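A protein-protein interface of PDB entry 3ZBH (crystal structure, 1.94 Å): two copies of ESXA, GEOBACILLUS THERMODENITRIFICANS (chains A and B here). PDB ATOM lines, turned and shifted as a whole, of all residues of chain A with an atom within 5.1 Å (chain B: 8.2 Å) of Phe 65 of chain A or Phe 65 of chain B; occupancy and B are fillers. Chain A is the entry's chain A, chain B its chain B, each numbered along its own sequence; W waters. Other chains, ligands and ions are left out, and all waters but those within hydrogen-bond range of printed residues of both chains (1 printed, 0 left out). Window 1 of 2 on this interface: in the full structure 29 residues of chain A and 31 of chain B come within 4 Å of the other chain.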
ATOM      1  N   VAL A  28     -27.653  28.643   3.976  1.00  0.00           N
ATOM      2  CA  VAL A  28     -27.375  27.446   3.178  1.00  0.00           C
ATOM      3  C   VAL A  28     -28.112  26.229   3.752  1.00  0.00           C
ATOM      4  O   VAL A  28     -28.700  25.442   3.012  1.00  0.00           O
ATOM      5  CB  VAL A  28     -25.861  27.141   3.024  1.00  0.00           C
ATOM      6  CG1 VAL A  28     -25.642  25.804   2.337  1.00  0.00           C
ATOM      7  CG2 VAL A  28     -25.147  28.243   2.210  1.00  0.00           C
ATOM      8  N   LEU A  31     -31.798  26.751   3.014  1.00  0.00           N
ATOM      9  CA  LEU A  31     -31.997  26.439   1.586  1.00  0.00           C
ATOM     10  C   LEU A  31     -32.091  24.931   1.321  1.00  0.00           C
ATOM     11  O   LEU A  31     -33.020  24.488   0.645  1.00  0.00           O
ATOM     12  CB  LEU A  31     -30.869  27.035   0.742  1.00  0.00           C
ATOM     13  CG  LEU A  31     -30.896  26.772  -0.769  1.00  0.00           C
ATOM     14  CD1 LEU A  31     -32.213  27.243  -1.388  1.00  0.00           C
ATOM     15  CD2 LEU A  31     -29.713  27.487  -1.401  1.00  0.00           C
ATOM     16  N   ILE A  32     -31.130  24.160   1.838  1.00  0.00           N
ATOM     17  CA  ILE A  32     -31.136  22.709   1.680  1.00  0.00           C
ATOM     18  C   ILE A  32     -32.458  22.128   2.167  1.00  0.00           C
ATOM     19  O   ILE A  32     -32.980  21.211   1.535  1.00  0.00           O
ATOM     20  CB  ILE A  32     -29.961  22.004   2.395  1.00  0.00           C
ATOM     21  CG1 ILE A  32     -28.624  22.462   1.836  1.00  0.00           C
ATOM     22  CG2 ILE A  32     -30.027  20.482   2.239  1.00  0.00           C
ATOM     23  CD1 ILE A  32     -27.501  22.330   2.854  1.00  0.00           C
ATOM     24  N   LEU A  35     -35.207  22.890  -0.349  1.00  0.00           N
ATOM     25  CA  LEU A  35     -34.999  22.092  -1.573  1.00  0.00           C
ATOM     26  C   LEU A  35     -35.344  20.600  -1.340  1.00  0.00           C
ATOM     27  O   LEU A  35     -35.864  19.920  -2.215  1.00  0.00           O
ATOM     28  CB  LEU A  35     -33.546  22.217  -2.022  1.00  0.00           C
ATOM     29  CG  LEU A  35     -33.178  23.575  -2.652  1.00  0.00           C
ATOM     30  CD1 LEU A  35     -31.754  23.494  -3.187  1.00  0.00           C
ATOM     31  CD2 LEU A  35     -34.189  23.972  -3.734  1.00  0.00           C
ATOM     32  N   LEU A  61     -25.669  16.983  -6.169  1.00  0.00           N
ATOM     33  CA  LEU A  61     -25.189  18.325  -5.810  1.00  0.00           C
ATOM     34  C   LEU A  61     -25.326  18.649  -4.309  1.00  0.00           C
ATOM     35  O   LEU A  61     -24.521  19.418  -3.731  1.00  0.00           O
ATOM     36  CB  LEU A  61     -25.932  19.356  -6.683  1.00  0.00           C
ATOM     37  CG  LEU A  61     -25.648  19.238  -8.194  1.00  0.00           C
ATOM     38  CD1 LEU A  61     -26.656  20.098  -8.969  1.00  0.00           C
ATOM     39  CD2 LEU A  61     -24.214  19.614  -8.568  1.00  0.00           C
ATOM     40  N   ARG A  62     -26.341  18.049  -3.680  1.00  0.00           N
ATOM     41  CA  ARG A  62     -26.643  18.228  -2.263  1.00  0.00           C
ATOM     42  C   ARG A  62     -25.416  18.153  -1.319  1.00  0.00           C
ATOM     43  O   ARG A  62     -25.263  19.046  -0.487  1.00  0.00           O
ATOM     44  CB  ARG A  62     -27.738  17.247  -1.801  1.00  0.00           C
ATOM     45  CG  ARG A  62     -28.665  17.808  -0.728  1.00  0.00           C
ATOM     46  CD  ARG A  62     -29.579  16.746  -0.121  1.00  0.00           C
ATOM     47  NE  ARG A  62     -28.921  16.186   1.050  1.00  0.00           N
ATOM     48  CZ  ARG A  62     -29.212  16.494   2.309  1.00  0.00           C
ATOM     49  NH1 ARG A  62     -30.195  17.323   2.601  1.00  0.00           N
ATOM     50  NH2 ARG A  62     -28.516  15.950   3.277  1.00  0.00           N
ATOM     51  N   PRO A  63     -24.547  17.123  -1.453  1.00  0.00           N
ATOM     52  CA  PRO A  63     -23.352  17.043  -0.571  1.00  0.00           C
ATOM     53  C   PRO A  63     -22.483  18.314  -0.593  1.00  0.00           C
ATOM     54  O   PRO A  63     -21.981  18.740   0.452  1.00  0.00           O
ATOM     55  CB  PRO A  63     -22.550  15.866  -1.151  1.00  0.00           C
ATOM     56  CG  PRO A  63     -23.549  15.038  -1.873  1.00  0.00           C
ATOM     57  CD  PRO A  63     -24.628  15.958  -2.363  1.00  0.00           C
ATOM     58  N   SER A  64     -22.322  18.917  -1.770  1.00  0.00           N
ATOM     59  CA  SER A  64     -21.605  20.216  -1.878  1.00  0.00           C
ATOM     60  C   SER A  64     -22.203  21.337  -1.054  1.00  0.00           C
ATOM     61  O   SER A  64     -21.465  22.138  -0.484  1.00  0.00           O
ATOM     62  CB  SER A  64     -21.450  20.625  -3.332  1.00  0.00           C
ATOM     63  OG  SER A  64     -20.742  19.607  -4.011  1.00  0.00           O
ATOM     64  N   PHE A  65     -23.534  21.400  -0.992  1.00  0.00           N
ATOM     65  CA  PHE A  65     -24.238  22.363  -0.153  1.00  0.00           C
ATOM     66  C   PHE A  65     -24.025  22.136   1.342  1.00  0.00           C
ATOM     67  O   PHE A  65     -23.842  23.097   2.097  1.00  0.00           O
ATOM     68  CB  PHE A  65     -25.738  22.389  -0.486  1.00  0.00           C
ATOM     69  CG  PHE A  65     -26.055  23.180  -1.735  1.00  0.00           C
ATOM     70  CD1 PHE A  65     -25.486  22.822  -2.950  1.00  0.00           C
ATOM     71  CD2 PHE A  65     -26.901  24.272  -1.685  1.00  0.00           C
ATOM     72  CE1 PHE A  65     -25.729  23.561  -4.104  1.00  0.00           C
ATOM     73  CE2 PHE A  65     -27.170  25.005  -2.843  1.00  0.00           C
ATOM     74  CZ  PHE A  65     -26.566  24.651  -4.047  1.00  0.00           C
ATOM     75  N   GLU A  66     -24.073  20.869   1.776  1.00  0.00           N
ATOM     76  CA  GLU A  66     -23.788  20.550   3.180  1.00  0.00           C
ATOM     77  C   GLU A  66     -22.370  20.985   3.547  1.00  0.00           C
ATOM     78  O   GLU A  66     -22.180  21.624   4.585  1.00  0.00           O
ATOM     79  CB  GLU A  66     -24.054  19.050   3.511  1.00  0.00           C
ATOM     80  CG  GLU A  66     -25.513  18.634   3.353  1.00  0.00           C
ATOM     81  CD  GLU A  66     -26.392  19.027   4.533  1.00  0.00           C
ATOM     82  OE1 GLU A  66     -25.881  19.634   5.500  1.00  0.00           O
ATOM     83  OE2 GLU A  66     -27.610  18.725   4.506  1.00  0.00           O
ATOM     84  N   LYS A  67     -21.402  20.683   2.682  1.00  0.00           N
ATOM     85  CA  LYS A  67     -20.003  21.079   2.885  1.00  0.00           C
ATOM     86  C   LYS A  67     -19.864  22.606   2.988  1.00  0.00           C
ATOM     87  O   LYS A  67     -19.174  23.113   3.884  1.00  0.00           O
ATOM     88  CB  LYS A  67     -19.106  20.556   1.769  1.00  0.00           C
ATOM     89  CG  LYS A  67     -18.614  19.136   1.999  1.00  0.00           C
ATOM     90  CD  LYS A  67     -17.362  18.808   1.191  1.00  0.00           C
ATOM     91  CE  LYS A  67     -17.679  18.246  -0.192  1.00  0.00           C
ATOM     92  NZ  LYS A  67     -18.380  16.924  -0.189  1.00  0.00           N
ATOM     93  N   MET A  68     -20.535  23.327   2.090  1.00  0.00           N
ATOM     94  CA  MET A  68     -20.507  24.804   2.142  1.00  0.00           C
ATOM     95  C   MET A  68     -21.009  25.330   3.473  1.00  0.00           C
ATOM     96  O   MET A  68     -20.373  26.176   4.072  1.00  0.00           O
ATOM     97  CB  MET A  68     -21.300  25.434   0.978  1.00  0.00           C
ATOM     98  CG  MET A  68     -21.237  26.960   0.964  1.00  0.00           C
ATOM     99  SD  MET A  68     -19.615  27.497   0.364  1.00  0.00           S
ATOM    100  CE  MET A  68     -19.791  27.281  -1.418  1.00  0.00           C
ATOM    101  N   ALA A  69     -22.148  24.833   3.963  1.00  0.00           N
ATOM    102  CA  ALA A  69     -22.630  25.303   5.268  1.00  0.00           C
ATOM    103  C   ALA A  69     -21.603  25.038   6.379  1.00  0.00           C
ATOM    104  O   ALA A  69     -21.439  25.892   7.249  1.00  0.00           O
ATOM    105  CB  ALA A  69     -23.986  24.714   5.628  1.00  0.00           C
ATOM    106  N   GLU B  24     -35.816  29.768  -5.737  1.00  0.00           N
ATOM    107  CA  GLU B  24     -34.630  29.188  -5.113  1.00  0.00           C
ATOM    108  C   GLU B  24     -33.409  29.284  -6.031  1.00  0.00           C
ATOM    109  O   GLU B  24     -32.294  29.450  -5.547  1.00  0.00           O
ATOM    110  CB  GLU B  24     -34.876  27.756  -4.583  1.00  0.00           C
ATOM    111  CG  GLU B  24     -35.951  27.624  -3.490  1.00  0.00           C
ATOM    112  CD  GLU B  24     -35.787  28.569  -2.281  1.00  0.00           C
ATOM    113  OE1 GLU B  24     -34.716  29.187  -2.067  1.00  0.00           O
ATOM    114  OE2 GLU B  24     -36.761  28.715  -1.518  1.00  0.00           O
ATOM    115  N   SER B  25     -33.607  29.250  -7.354  1.00  0.00           N
ATOM    116  CA  SER B  25     -32.489  29.478  -8.246  1.00  0.00           C
ATOM    117  C   SER B  25     -31.888  30.888  -7.985  1.00  0.00           C
ATOM    118  O   SER B  25     -30.667  31.017  -7.880  1.00  0.00           O
ATOM    119  CB  SER B  25     -32.886  29.363  -9.715  1.00  0.00           C
ATOM    120  OG  SER B  25     -31.762  29.708 -10.516  1.00  0.00           O
ATOM    121  N   ASN B  27     -32.115  32.769  -5.219  1.00  0.00           N
ATOM    122  CA  ASN B  27     -31.425  32.692  -3.949  1.00  0.00           C
ATOM    123  C   ASN B  27     -30.024  32.087  -4.012  1.00  0.00           C
ATOM    124  O   ASN B  27     -29.139  32.557  -3.295  1.00  0.00           O
ATOM    125  CB  ASN B  27     -32.263  31.955  -2.895  1.00  0.00           C
ATOM    126  CG  ASN B  27     -33.565  32.674  -2.574  1.00  0.00           C
ATOM    127  OD1 ASN B  27     -33.663  33.881  -2.716  1.00  0.00           O
ATOM    128  ND2 ASN B  27     -34.568  31.924  -2.165  1.00  0.00           N
ATOM    129  N   VAL B  28     -29.821  31.057  -4.849  1.00  0.00           N
ATOM    130  CA  VAL B  28     -28.492  30.457  -5.050  1.00  0.00           C
ATOM    131  C   VAL B  28     -27.492  31.445  -5.674  1.00  0.00           C
ATOM    132  O   VAL B  28     -26.382  31.601  -5.148  1.00  0.00           O
ATOM    133  CB  VAL B  28     -28.529  29.117  -5.875  1.00  0.00           C
ATOM    134  CG1 VAL B  28     -27.121  28.641  -6.283  1.00  0.00           C
ATOM    135  CG2 VAL B  28     -29.213  28.044  -5.062  1.00  0.00           C
ATOM    136  N   THR B  29     -27.861  32.115  -6.779  1.00  0.00           N
ATOM    137  CA  THR B  29     -26.900  33.023  -7.408  1.00  0.00           C
ATOM    138  C   THR B  29     -26.653  34.285  -6.564  1.00  0.00           C
ATOM    139  O   THR B  29     -25.504  34.752  -6.474  1.00  0.00           O
ATOM    140  CB  THR B  29     -27.250  33.392  -8.873  1.00  0.00           C
ATOM    141  OG1 THR B  29     -28.587  33.862  -8.930  1.00  0.00           O
ATOM    142  CG2 THR B  29     -27.072  32.152  -9.800  1.00  0.00           C
ATOM    143  N   LEU B  31     -26.708  34.308  -3.298  1.00  0.00           N
ATOM    144  CA  LEU B  31     -25.802  33.823  -2.261  1.00  0.00           C
ATOM    145  C   LEU B  31     -24.366  33.707  -2.765  1.00  0.00           C
ATOM    146  O   LEU B  31     -23.431  34.152  -2.112  1.00  0.00           O
ATOM    147  CB  LEU B  31     -26.304  32.465  -1.736  1.00  0.00           C
ATOM    148  CG  LEU B  31     -25.408  31.627  -0.835  1.00  0.00           C
ATOM    149  CD1 LEU B  31     -25.261  32.242   0.559  1.00  0.00           C
ATOM    150  CD2 LEU B  31     -26.057  30.244  -0.746  1.00  0.00           C
ATOM    151  N   ILE B  32     -24.175  33.130  -3.930  1.00  0.00           N
ATOM    152  CA  ILE B  32     -22.835  33.044  -4.481  1.00  0.00           C
ATOM    153  C   ILE B  32     -22.175  34.423  -4.649  1.00  0.00           C
ATOM    154  O   ILE B  32     -21.031  34.620  -4.265  1.00  0.00           O
ATOM    155  CB  ILE B  32     -22.803  32.238  -5.787  1.00  0.00           C
ATOM    156  CG1 ILE B  32     -23.116  30.758  -5.495  1.00  0.00           C
ATOM    157  CG2 ILE B  32     -21.424  32.348  -6.442  1.00  0.00           C
ATOM    158  CD1 ILE B  32     -22.258  30.138  -4.379  1.00  0.00           C
ATOM    159  N   LEU B  35     -21.195  35.584  -1.124  1.00  0.00           N
ATOM    160  CA  LEU B  35     -19.996  34.838  -0.731  1.00  0.00           C
ATOM    161  C   LEU B  35     -18.759  35.212  -1.565  1.00  0.00           C
ATOM    162  O   LEU B  35     -17.655  35.189  -1.056  1.00  0.00           O
ATOM    163  CB  LEU B  35     -20.238  33.328  -0.832  1.00  0.00           C
ATOM    164  CG  LEU B  35     -21.350  32.778   0.071  1.00  0.00           C
ATOM    165  CD1 LEU B  35     -21.449  31.268  -0.160  1.00  0.00           C
ATOM    166  CD2 LEU B  35     -21.038  33.077   1.535  1.00  0.00           C
ATOM    167  N   TYR B  58     -13.736  26.904  -0.917  1.00  0.00           N
ATOM    168  CA  TYR B  58     -14.820  27.691  -1.497  1.00  0.00           C
ATOM    169  C   TYR B  58     -14.900  27.530  -3.019  1.00  0.00           C
ATOM    170  O   TYR B  58     -15.958  27.148  -3.572  1.00  0.00           O
ATOM    171  CB  TYR B  58     -14.679  29.174  -1.119  1.00  0.00           C
ATOM    172  CG  TYR B  58     -15.731  30.005  -1.804  1.00  0.00           C
ATOM    173  CD1 TYR B  58     -17.063  29.839  -1.468  1.00  0.00           C
ATOM    174  CD2 TYR B  58     -15.401  30.915  -2.825  1.00  0.00           C
ATOM    175  CE1 TYR B  58     -18.064  30.561  -2.089  1.00  0.00           C
ATOM    176  CE2 TYR B  58     -16.400  31.674  -3.443  1.00  0.00           C
ATOM    177  CZ  TYR B  58     -17.728  31.478  -3.076  1.00  0.00           C
ATOM    178  OH  TYR B  58     -18.758  32.158  -3.669  1.00  0.00           O
ATOM    179  N   GLU B  60     -13.662  25.236  -4.845  1.00  0.00           N
ATOM    180  CA  GLU B  60     -13.992  23.849  -5.188  1.00  0.00           C
ATOM    181  C   GLU B  60     -15.512  23.601  -5.200  1.00  0.00           C
ATOM    182  O   GLU B  60     -16.017  22.786  -5.975  1.00  0.00           O
ATOM    183  CB  GLU B  60     -13.293  22.886  -4.212  1.00  0.00           C
ATOM    184  CG  GLU B  60     -13.141  21.458  -4.720  1.00  0.00           C
ATOM    185  CD  GLU B  60     -14.217  20.516  -4.201  1.00  0.00           C
ATOM    186  OE1 GLU B  60     -14.366  20.397  -2.962  1.00  0.00           O
ATOM    187  OE2 GLU B  60     -14.912  19.882  -5.032  1.00  0.00           O
ATOM    188  N   LEU B  61     -16.239  24.304  -4.340  1.00  0.00           N
ATOM    189  CA  LEU B  61     -17.659  24.056  -4.174  1.00  0.00           C
ATOM    190  C   LEU B  61     -18.526  24.953  -5.043  1.00  0.00           C
ATOM    191  O   LEU B  61     -19.656  24.602  -5.388  1.00  0.00           O
ATOM    192  CB  LEU B  61     -18.056  24.256  -2.713  1.00  0.00           C
ATOM    193  CG  LEU B  61     -17.434  23.277  -1.720  1.00  0.00           C
ATOM    194  CD1 LEU B  61     -17.765  23.725  -0.305  1.00  0.00           C
ATOM    195  CD2 LEU B  61     -17.925  21.860  -1.979  1.00  0.00           C
ATOM    196  N   ARG B  62     -18.004  26.119  -5.371  1.00  0.00           N
ATOM    197  CA  ARG B  62     -18.758  27.119  -6.112  1.00  0.00           C
ATOM    198  C   ARG B  62     -19.381  26.569  -7.411  1.00  0.00           C
ATOM    199  O   ARG B  62     -20.529  26.868  -7.695  1.00  0.00           O
ATOM    200  CB  ARG B  62     -17.877  28.331  -6.391  1.00  0.00           C
ATOM    201  CG  ARG B  62     -18.650  29.603  -6.759  1.00  0.00           C
ATOM    202  CD  ARG B  62     -17.639  30.660  -7.219  1.00  0.00           C
ATOM    203  NE  ARG B  62     -18.288  31.890  -7.646  1.00  0.00           N
ATOM    204  CZ  ARG B  62     -18.698  32.137  -8.889  1.00  0.00           C
ATOM    205  NH1 ARG B  62     -18.550  31.226  -9.860  1.00  0.00           N
ATOM    206  NH2 ARG B  62     -19.275  33.298  -9.160  1.00  0.00           N
ATOM    207  N   PRO B  63     -18.631  25.765  -8.205  1.00  0.00           N
ATOM    208  CA  PRO B  63     -19.249  25.372  -9.466  1.00  0.00           C
ATOM    209  C   PRO B  63     -20.508  24.502  -9.271  1.00  0.00           C
ATOM    210  O   PRO B  63     -21.374  24.484 -10.152  1.00  0.00           O
ATOM    211  CB  PRO B  63     -18.166  24.554 -10.178  1.00  0.00           C
ATOM    212  CG  PRO B  63     -16.879  24.898  -9.508  1.00  0.00           C
ATOM    213  CD  PRO B  63     -17.197  25.404  -8.133  1.00  0.00           C
ATOM    214  N   SER B  64     -20.602  23.809  -8.139  1.00  0.00           N
ATOM    215  CA  SER B  64     -21.748  22.951  -7.890  1.00  0.00           C
ATOM    216  C   SER B  64     -22.964  23.801  -7.534  1.00  0.00           C
ATOM    217  O   SER B  64     -24.093  23.396  -7.763  1.00  0.00           O
ATOM    218  CB  SER B  64     -21.430  21.970  -6.768  1.00  0.00           C
ATOM    219  OG  SER B  64     -20.486  21.017  -7.233  1.00  0.00           O
ATOM    220  N   PHE B  65     -22.728  24.979  -6.948  1.00  0.00           N
ATOM    221  CA  PHE B  65     -23.809  25.929  -6.741  1.00  0.00           C
ATOM    222  C   PHE B  65     -24.331  26.468  -8.071  1.00  0.00           C
ATOM    223  O   PHE B  65     -25.531  26.650  -8.218  1.00  0.00           O
ATOM    224  CB  PHE B  65     -23.392  27.075  -5.774  1.00  0.00           C
ATOM    225  CG  PHE B  65     -23.426  26.673  -4.315  1.00  0.00           C
ATOM    226  CD1 PHE B  65     -22.600  25.672  -3.827  1.00  0.00           C
ATOM    227  CD2 PHE B  65     -24.320  27.280  -3.434  1.00  0.00           C
ATOM    228  CE1 PHE B  65     -22.657  25.279  -2.491  1.00  0.00           C
ATOM    229  CE2 PHE B  65     -24.372  26.898  -2.101  1.00  0.00           C
ATOM    230  CZ  PHE B  65     -23.549  25.889  -1.625  1.00  0.00           C
ATOM    231  N   GLU B  66     -23.449  26.724  -9.036  1.00  0.00           N
ATOM    232  CA  GLU B  66     -23.927  27.203 -10.345  1.00  0.00           C
ATOM    233  C   GLU B  66     -24.710  26.088 -11.023  1.00  0.00           C
ATOM    234  O   GLU B  66     -25.690  26.337 -11.684  1.00  0.00           O
ATOM    235  CB  GLU B  66     -22.770  27.663 -11.240  1.00  0.00           C
ATOM    236  CG  GLU B  66     -21.989  28.869 -10.671  1.00  0.00           C
ATOM    237  CD  GLU B  66     -22.870  30.078 -10.336  1.00  0.00           C
ATOM    238  OE1 GLU B  66     -23.956  30.271 -10.939  1.00  0.00           O
ATOM    239  OE2 GLU B  66     -22.488  30.864  -9.434  1.00  0.00           O
ATOM    240  N   LYS B  67     -24.279  24.840 -10.835  1.00  0.00           N
ATOM    241  CA  LYS B  67     -25.038  23.720 -11.392  1.00  0.00           C
ATOM    242  C   LYS B  67     -26.414  23.603 -10.751  1.00  0.00           C
ATOM    243  O   LYS B  67     -27.382  23.246 -11.401  1.00  0.00           O
ATOM    244  CB  LYS B  67     -24.265  22.406 -11.216  1.00  0.00           C
ATOM    245  CG  LYS B  67     -23.123  22.198 -12.199  1.00  0.00           C
ATOM    246  CD  LYS B  67     -22.194  21.119 -11.675  1.00  0.00           C
ATOM    247  CE  LYS B  67     -20.864  21.031 -12.408  1.00  0.00           C
ATOM    248  NZ  LYS B  67     -21.054  20.362 -13.724  1.00  0.00           N
ATOM    249  N   MET B  68     -26.500  23.870  -9.457  1.00  0.00           N
ATOM    250  CA  MET B  68     -27.795  23.826  -8.785  1.00  0.00           C
ATOM    251  C   MET B  68     -28.704  24.912  -9.358  1.00  0.00           C
ATOM    252  O   MET B  68     -29.881  24.694  -9.582  1.00  0.00           O
ATOM    253  CB  MET B  68     -27.631  24.003  -7.280  1.00  0.00           C
ATOM    254  CG  MET B  68     -28.942  23.903  -6.520  1.00  0.00           C
ATOM    255  SD  MET B  68     -29.563  22.200  -6.441  1.00  0.00           S
ATOM    256  CE  MET B  68     -28.590  21.595  -5.060  1.00  0.00           C
ATOM    257  N   ALA B  69     -28.154  26.111  -9.538  1.00  0.00           N
ATOM    258  CA  ALA B  69     -28.960  27.192 -10.082  1.00  0.00           C
ATOM    259  C   ALA B  69     -29.494  26.833 -11.487  1.00  0.00           C
ATOM    260  O   ALA B  69     -30.669  27.077 -11.786  1.00  0.00           O
ATOM    261  CB  ALA B  69     -28.162  28.504 -10.073  1.00  0.00           C
ATOM    262  N   VAL B  70     -28.676  26.218 -12.330  1.00  0.00           N
ATOM    263  CA  VAL B  70     -29.160  25.790 -13.648  1.00  0.00           C
ATOM    264  C   VAL B  70     -30.274  24.753 -13.473  1.00  0.00           C
ATOM    265  O   VAL B  70     -31.355  24.857 -14.073  1.00  0.00           O
ATOM    266  CB  VAL B  70     -28.017  25.184 -14.496  1.00  0.00           C
ATOM    267  CG1 VAL B  70     -28.559  24.468 -15.722  1.00  0.00           C
ATOM    268  CG2 VAL B  70     -27.014  26.268 -14.915  1.00  0.00           C
ATOM    269  N   LEU B  71     -30.008  23.744 -12.648  1.00  0.00           N
ATOM    270  CA  LEU B  71     -31.015  22.669 -12.419  1.00  0.00           C
ATOM    271  C   LEU B  71     -32.360  23.204 -11.971  1.00  0.00           C
ATOM    272  O   LEU B  71     -33.389  22.833 -12.527  1.00  0.00           O
ATOM    273  CB  LEU B  71     -30.496  21.711 -11.339  1.00  0.00           C
ATOM    274  CG  LEU B  71     -31.487  20.671 -10.795  1.00  0.00           C
ATOM    275  CD1 LEU B  71     -31.823  19.739 -11.930  1.00  0.00           C
ATOM    276  CD2 LEU B  71     -30.793  19.927  -9.651  1.00  0.00           C
ATOM    277  N   LEU B  72     -32.357  24.074 -10.951  1.00  0.00           N
ATOM    278  CA  LEU B  72     -33.592  24.586 -10.395  1.00  0.00           C
ATOM    279  C   LEU B  72     -34.361  25.391 -11.438  1.00  0.00           C
ATOM    280  O   LEU B  72     -35.557  25.303 -11.512  1.00  0.00           O
ATOM    281  CB  LEU B  72     -33.332  25.462  -9.158  1.00  0.00           C
ATOM    282  CG  LEU B  72     -32.617  24.756  -7.971  1.00  0.00           C
ATOM    283  CD1 LEU B  72     -32.182  25.786  -6.938  1.00  0.00           C
ATOM    284  CD2 LEU B  72     -33.397  23.599  -7.333  1.00  0.00           C
HETATM  285  O   HOH W   1     -20.749  18.472  -6.896  1.00  0.00           O
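OH of Tyr 58 of chain B is in hydrogen-bond range of O of Ile 32 of chain B, 3.4 Å away.
The side-chain carboxylate (OE1) of Glu 24 of chain B sits at hydrogen-bond distance from the side-chain amide nitrogen (ND2) of Asn 27 of chain B (2.7 Å).
CD2 of Leu 31 of chain B touches CG2 of Val 28 of chain A (3.7 Å).
CD1 of Leu 31 of chain A touches OE1 of Glu 24 of chain B (3.2 Å).
CD2 of Leu 31 of chain A touches CG2 of Val 28 of chain B, 3.7 Å away.
Glu 24 of chain B touches Leu 35 of chain A.
Leu 72 of chain B touches Leu 35 of chain A.
CD2 of Leu 61 of chain A touches O of Ser 64 of chain B (3.9 Å).
Lys 67 of chain B touches Leu 61 of chain A (CB to CD2, 3.8 Å).
Ser 64 of chain A touches Leu 61 of chain B (O to CD2, 3.9 Å).
CE2 of Phe 65 of chain A touches CE2 of Phe 65 of chain B, 3.5 Å away.
CB of Met 68 of chain A touches CZ of Phe 65 of chain B (3.5 Å).
Leu 61 of chain A touches Lys 67 of chain B, but with the chains exchanged Lys 67 of chain A does not touch Leu 61 of chain B (4.02 Å).
Ser 64 of chain B touches its own counterpart, Ser 64 of chain A.
Ser 64 of chain A touches Phe 65 of chain B, but with the chains exchanged Phe 65 of chain A does not touch Ser 64 of chain B (4.01 Å).
Phe 65 of chain A touches its own counterpart, Phe 65 of chain B.
Water W1 lies within hydrogen-bond range of the side-chain hydroxyl of Ser 64 of chain B (2.6 Å) and the side-chain hydroxyl of Ser 64 of chain A (3.1 Å).
Of the 22 printed residues of chain B, 10 touch a printed residue of chain A.
Among the printed residues, 16 pairs touch across the chains.
Of the printed residues of chain B, Phe 65 of chain A touches Phe 65 and Met 68.
Glu 66 of chain A touches none of the printed residues of chain B.
Of the printed residues of chain A, Tyr 58 of chain B touches Met 68.
Phe 65 of chain B touches just these residues of chain A: Ser 64 (3.9 Å), Phe 65 (3.5 Å) and Met 68 (3.5 Å).
Printed residues of chain A within 4 Å of Met 68 of chain B: Leu 61 and Phe 65.
The nearest printed residue of chain B that does not touch Phe 65 of chain A is Ser 64 of chain B (4.01 Å).
The nearest residue of chain A that does not touch Phe 65 of chain B is Val 28 of chain A (4.5 Å).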
